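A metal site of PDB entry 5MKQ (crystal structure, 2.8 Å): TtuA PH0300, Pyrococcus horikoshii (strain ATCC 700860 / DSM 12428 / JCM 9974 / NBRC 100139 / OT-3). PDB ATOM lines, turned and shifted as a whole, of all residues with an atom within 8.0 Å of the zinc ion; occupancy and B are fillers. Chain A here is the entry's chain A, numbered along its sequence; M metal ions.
Of the 17 residues printed, 4 come within 4 Å of the zinc ion.
The nearest printed residue that does not touch the zinc ion is Phe 8 (4.6 Å).
The zinc ion is bound by the side-chain sulfur of Cys 6 (2.2 Å), the side-chain sulfur of Cys 9 (2.2 Å) and the side-chain sulfur of Cys 25 (2.5 Å).
The zinc ion has three donor atoms within binding distance.
Slightly farther from the zinc ion lies ND1 of His 28 (2.7 Å).
N of Phe 8 lies close to SG of Cys 6 (3.6 Å).
The backbone NH (N) of Cys 6 is in hydrogen-bond range of the backbone carbonyl oxygen (O) of Arg 11.
ND1 of His 28 lies close to SG of Cys 9 (3.7 Å).
N of His 28 lies close to SG of Cys 25.
The side-chain sulfur (SG) of Cys 25 sits close to the backbone NH (N) of Glu 27 (3.8 Å).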
ATOM      1  N   LYS A   5     -22.896  18.779   1.484  1.00  0.00           N
ATOM      2  CA  LYS A   5     -23.596  20.028   1.178  1.00  0.00           C
ATOM      3  C   LYS A   5     -24.349  19.907  -0.146  1.00  0.00           C
ATOM      4  O   LYS A   5     -23.999  19.042  -0.964  1.00  0.00           O
ATOM      5  CB  LYS A   5     -22.602  21.202   1.129  1.00  0.00           C
ATOM      6  CG  LYS A   5     -22.091  21.631   2.504  1.00  0.00           C
ATOM      7  CD  LYS A   5     -22.823  22.865   3.025  1.00  0.00           C
ATOM      8  CE  LYS A   5     -22.383  23.260   4.417  1.00  0.00           C
ATOM      9  NZ  LYS A   5     -23.076  22.439   5.453  1.00  0.00           N
ATOM     10  N   CYS A   6     -25.393  20.743  -0.360  1.00  0.00           N
ATOM     11  CA  CYS A   6     -26.195  20.725  -1.592  1.00  0.00           C
ATOM     12  C   CYS A   6     -25.395  21.124  -2.830  1.00  0.00           C
ATOM     13  O   CYS A   6     -24.539  22.002  -2.772  1.00  0.00           O
ATOM     14  CB  CYS A   6     -27.474  21.564  -1.451  1.00  0.00           C
ATOM     15  SG  CYS A   6     -28.596  21.451  -2.872  1.00  0.00           S
ATOM     16  N   LYS A   7     -25.697  20.451  -3.961  1.00  0.00           N
ATOM     17  CA  LYS A   7     -25.052  20.676  -5.246  1.00  0.00           C
ATOM     18  C   LYS A   7     -25.369  22.048  -5.869  1.00  0.00           C
ATOM     19  O   LYS A   7     -24.611  22.507  -6.718  1.00  0.00           O
ATOM     20  CB  LYS A   7     -25.404  19.546  -6.224  1.00  0.00           C
ATOM     21  CG  LYS A   7     -24.245  19.153  -7.135  1.00  0.00           C
ATOM     22  CD  LYS A   7     -24.607  17.952  -7.989  1.00  0.00           C
ATOM     23  CE  LYS A   7     -23.414  17.382  -8.718  1.00  0.00           C
ATOM     24  NZ  LYS A   7     -23.772  16.163  -9.491  1.00  0.00           N
ATOM     25  N   PHE A   8     -26.473  22.715  -5.422  1.00  0.00           N
ATOM     26  CA  PHE A   8     -26.897  24.005  -5.964  1.00  0.00           C
ATOM     27  C   PHE A   8     -26.886  25.167  -4.964  1.00  0.00           C
ATOM     28  O   PHE A   8     -27.003  26.328  -5.397  1.00  0.00           O
ATOM     29  CB  PHE A   8     -28.280  23.886  -6.619  1.00  0.00           C
ATOM     30  CG  PHE A   8     -28.383  22.800  -7.664  1.00  0.00           C
ATOM     31  CD1 PHE A   8     -27.834  22.963  -8.924  1.00  0.00           C
ATOM     32  CD2 PHE A   8     -29.027  21.597  -7.377  1.00  0.00           C
ATOM     33  CE1 PHE A   8     -27.917  21.937  -9.880  1.00  0.00           C
ATOM     34  CE2 PHE A   8     -29.115  20.579  -8.330  1.00  0.00           C
ATOM     35  CZ  PHE A   8     -28.558  20.768  -9.580  1.00  0.00           C
ATOM     36  N   CYS A   9     -26.744  24.900  -3.654  1.00  0.00           N
ATOM     37  CA  CYS A   9     -26.691  25.940  -2.635  1.00  0.00           C
ATOM     38  C   CYS A   9     -25.773  25.585  -1.437  1.00  0.00           C
ATOM     39  O   CYS A   9     -25.284  24.463  -1.340  1.00  0.00           O
ATOM     40  CB  CYS A   9     -28.089  26.358  -2.168  1.00  0.00           C
ATOM     41  SG  CYS A   9     -29.088  25.025  -1.466  1.00  0.00           S
ATOM     42  N   SER A  10     -25.550  26.566  -0.546  1.00  0.00           N
ATOM     43  CA  SER A  10     -24.717  26.464   0.671  1.00  0.00           C
ATOM     44  C   SER A  10     -25.406  25.681   1.807  1.00  0.00           C
ATOM     45  O   SER A  10     -24.805  25.516   2.873  1.00  0.00           O
ATOM     46  CB  SER A  10     -24.336  27.849   1.152  1.00  0.00           C
ATOM     47  OG  SER A  10     -25.482  28.568   1.576  1.00  0.00           O
ATOM     48  N   ARG A  11     -26.669  25.252   1.604  1.00  0.00           N
ATOM     49  CA  ARG A  11     -27.451  24.489   2.579  1.00  0.00           C
ATOM     50  C   ARG A  11     -26.924  23.059   2.671  1.00  0.00           C
ATOM     51  O   ARG A  11     -26.421  22.519   1.662  1.00  0.00           O
ATOM     52  CB  ARG A  11     -28.944  24.495   2.216  1.00  0.00           C
ATOM     53  CG  ARG A  11     -29.625  25.835   2.418  1.00  0.00           C
ATOM     54  CD  ARG A  11     -30.962  25.899   1.707  1.00  0.00           C
ATOM     55  NE  ARG A  11     -31.387  27.288   1.489  1.00  0.00           N
ATOM     56  CZ  ARG A  11     -32.441  27.637   0.770  1.00  0.00           C
ATOM     57  NH1 ARG A  11     -33.202  26.719   0.177  1.00  0.00           N
ATOM     58  NH2 ARG A  11     -32.758  28.917   0.631  1.00  0.00           N
ATOM     59  N   GLU A  12     -27.038  22.444   3.866  1.00  0.00           N
ATOM     60  CA  GLU A  12     -26.576  21.082   4.110  1.00  0.00           C
ATOM     61  C   GLU A  12     -27.426  20.038   3.382  1.00  0.00           C
ATOM     62  O   GLU A  12     -28.633  20.222   3.221  1.00  0.00           O
ATOM     63  CB  GLU A  12     -26.502  20.787   5.613  1.00  0.00           C
ATOM     64  CG  GLU A  12     -25.460  19.740   5.957  1.00  0.00           C
ATOM     65  CD  GLU A  12     -25.493  19.147   7.357  1.00  0.00           C
ATOM     66  OE1 GLU A  12     -26.524  19.277   8.049  1.00  0.00           O
ATOM     67  OE2 GLU A  12     -24.485  18.497   7.738  1.00  0.00           O
ATOM     68  N   ALA A  13     -26.774  18.961   2.901  1.00  0.00           N
ATOM     69  CA  ALA A  13     -27.411  17.862   2.182  1.00  0.00           C
ATOM     70  C   ALA A  13     -28.475  17.166   3.031  1.00  0.00           C
ATOM     71  O   ALA A  13     -28.286  16.974   4.236  1.00  0.00           O
ATOM     72  CB  ALA A  13     -26.367  16.859   1.714  1.00  0.00           C
ATOM     73  N   TYR A  14     -29.596  16.819   2.388  1.00  0.00           N
ATOM     74  CA  TYR A  14     -30.737  16.147   2.995  1.00  0.00           C
ATOM     75  C   TYR A  14     -30.797  14.697   2.530  1.00  0.00           C
ATOM     76  O   TYR A  14     -31.028  13.800   3.334  1.00  0.00           O
ATOM     77  CB  TYR A  14     -32.030  16.915   2.656  1.00  0.00           C
ATOM     78  CG  TYR A  14     -33.330  16.252   3.042  1.00  0.00           C
ATOM     79  CD1 TYR A  14     -33.686  16.109   4.389  1.00  0.00           C
ATOM     80  CD2 TYR A  14     -34.256  15.857   2.086  1.00  0.00           C
ATOM     81  CE1 TYR A  14     -34.904  15.536   4.746  1.00  0.00           C
ATOM     82  CE2 TYR A  14     -35.471  15.287   2.434  1.00  0.00           C
ATOM     83  CZ  TYR A  14     -35.789  15.123   3.769  1.00  0.00           C
ATOM     84  OH  TYR A  14     -36.989  14.558   4.133  1.00  0.00           O
ATOM     85  N   TYR A  23     -26.042  15.375  -4.263  1.00  0.00           N
ATOM     86  CA  TYR A  23     -26.474  15.682  -2.903  1.00  0.00           C
ATOM     87  C   TYR A  23     -27.364  16.919  -2.926  1.00  0.00           C
ATOM     88  O   TYR A  23     -26.927  17.986  -3.397  1.00  0.00           O
ATOM     89  CB  TYR A  23     -25.278  15.846  -1.955  1.00  0.00           C
ATOM     90  CG  TYR A  23     -24.602  14.539  -1.566  1.00  0.00           C
ATOM     91  CD1 TYR A  23     -23.687  13.929  -2.415  1.00  0.00           C
ATOM     92  CD2 TYR A  23     -24.880  13.929  -0.346  1.00  0.00           C
ATOM     93  CE1 TYR A  23     -23.064  12.730  -2.062  1.00  0.00           C
ATOM     94  CE2 TYR A  23     -24.247  12.743   0.024  1.00  0.00           C
ATOM     95  CZ  TYR A  23     -23.341  12.145  -0.845  1.00  0.00           C
ATOM     96  OH  TYR A  23     -22.720  10.960  -0.509  1.00  0.00           O
ATOM     97  N   LEU A  24     -28.616  16.776  -2.479  1.00  0.00           N
ATOM     98  CA  LEU A  24     -29.628  17.841  -2.478  1.00  0.00           C
ATOM     99  C   LEU A  24     -30.149  18.135  -1.084  1.00  0.00           C
ATOM    100  O   LEU A  24     -30.299  17.213  -0.273  1.00  0.00           O
ATOM    101  CB  LEU A  24     -30.814  17.459  -3.381  1.00  0.00           C
ATOM    102  CG  LEU A  24     -30.541  17.279  -4.867  1.00  0.00           C
ATOM    103  CD1 LEU A  24     -31.507  16.292  -5.479  1.00  0.00           C
ATOM    104  CD2 LEU A  24     -30.611  18.609  -5.598  1.00  0.00           C
ATOM    105  N   CYS A  25     -30.492  19.410  -0.820  1.00  0.00           N
ATOM    106  CA  CYS A  25     -31.086  19.861   0.431  1.00  0.00           C
ATOM    107  C   CYS A  25     -32.609  19.670   0.328  1.00  0.00           C
ATOM    108  O   CYS A  25     -33.100  19.284  -0.738  1.00  0.00           O
ATOM    109  CB  CYS A  25     -30.719  21.320   0.720  1.00  0.00           C
ATOM    110  SG  CYS A  25     -31.522  22.522  -0.376  1.00  0.00           S
ATOM    111  N   GLU A  26     -33.357  19.926   1.429  1.00  0.00           N
ATOM    112  CA  GLU A  26     -34.823  19.788   1.483  1.00  0.00           C
ATOM    113  C   GLU A  26     -35.528  20.505   0.333  1.00  0.00           C
ATOM    114  O   GLU A  26     -36.344  19.886  -0.358  1.00  0.00           O
ATOM    115  CB  GLU A  26     -35.374  20.304   2.820  1.00  0.00           C
ATOM    116  CG  GLU A  26     -35.321  19.305   3.954  1.00  0.00           C
ATOM    117  CD  GLU A  26     -36.013  19.779   5.217  1.00  0.00           C
ATOM    118  OE1 GLU A  26     -37.063  19.189   5.557  1.00  0.00           O
ATOM    119  OE2 GLU A  26     -35.538  20.761   5.832  1.00  0.00           O
ATOM    120  N   GLU A  27     -35.213  21.799   0.146  1.00  0.00           N
ATOM    121  CA  GLU A  27     -35.825  22.678  -0.866  1.00  0.00           C
ATOM    122  C   GLU A  27     -35.497  22.305  -2.302  1.00  0.00           C
ATOM    123  O   GLU A  27     -36.352  22.466  -3.179  1.00  0.00           O
ATOM    124  CB  GLU A  27     -35.482  24.158  -0.574  1.00  0.00           C
ATOM    125  CG  GLU A  27     -35.942  24.662   0.785  1.00  0.00           C
ATOM    126  CD  GLU A  27     -37.370  24.330   1.199  1.00  0.00           C
ATOM    127  OE1 GLU A  27     -38.299  24.636   0.423  1.00  0.00           O
ATOM    128  OE2 GLU A  27     -37.554  23.779   2.306  1.00  0.00           O
ATOM    129  N   HIS A  28     -34.272  21.814  -2.546  1.00  0.00           N
ATOM    130  CA  HIS A  28     -33.844  21.403  -3.879  1.00  0.00           C
ATOM    131  C   HIS A  28     -34.325  20.014  -4.240  1.00  0.00           C
ATOM    132  O   HIS A  28     -34.543  19.736  -5.432  1.00  0.00           O
ATOM    133  CB  HIS A  28     -32.334  21.534  -4.046  1.00  0.00           C
ATOM    134  CG  HIS A  28     -31.948  22.880  -4.568  1.00  0.00           C
ATOM    135  ND1 HIS A  28     -31.857  23.973  -3.728  1.00  0.00           N
ATOM    136  CD2 HIS A  28     -31.711  23.277  -5.838  1.00  0.00           C
ATOM    137  CE1 HIS A  28     -31.544  24.994  -4.506  1.00  0.00           C
ATOM    138  NE2 HIS A  28     -31.442  24.627  -5.778  1.00  0.00           N
ATOM    139  N   PHE A  29     -34.498  19.138  -3.234  1.00  0.00           N
ATOM    140  CA  PHE A  29     -35.000  17.785  -3.457  1.00  0.00           C
ATOM    141  C   PHE A  29     -36.471  17.828  -3.867  1.00  0.00           C
ATOM    142  O   PHE A  29     -36.857  17.120  -4.811  1.00  0.00           O
ATOM    143  CB  PHE A  29     -34.804  16.892  -2.216  1.00  0.00           C
ATOM    144  CG  PHE A  29     -35.535  15.575  -2.308  1.00  0.00           C
ATOM    145  CD1 PHE A  29     -35.173  14.620  -3.263  1.00  0.00           C
ATOM    146  CD2 PHE A  29     -36.600  15.295  -1.475  1.00  0.00           C
ATOM    147  CE1 PHE A  29     -35.862  13.413  -3.362  1.00  0.00           C
ATOM    148  CE2 PHE A  29     -37.301  14.095  -1.585  1.00  0.00           C
ATOM    149  CZ  PHE A  29     -36.920  13.158  -2.519  1.00  0.00           C
HETATM  150 ZN    ZN M   1     -29.814  23.083  -2.141  1.00  0.00          ZN
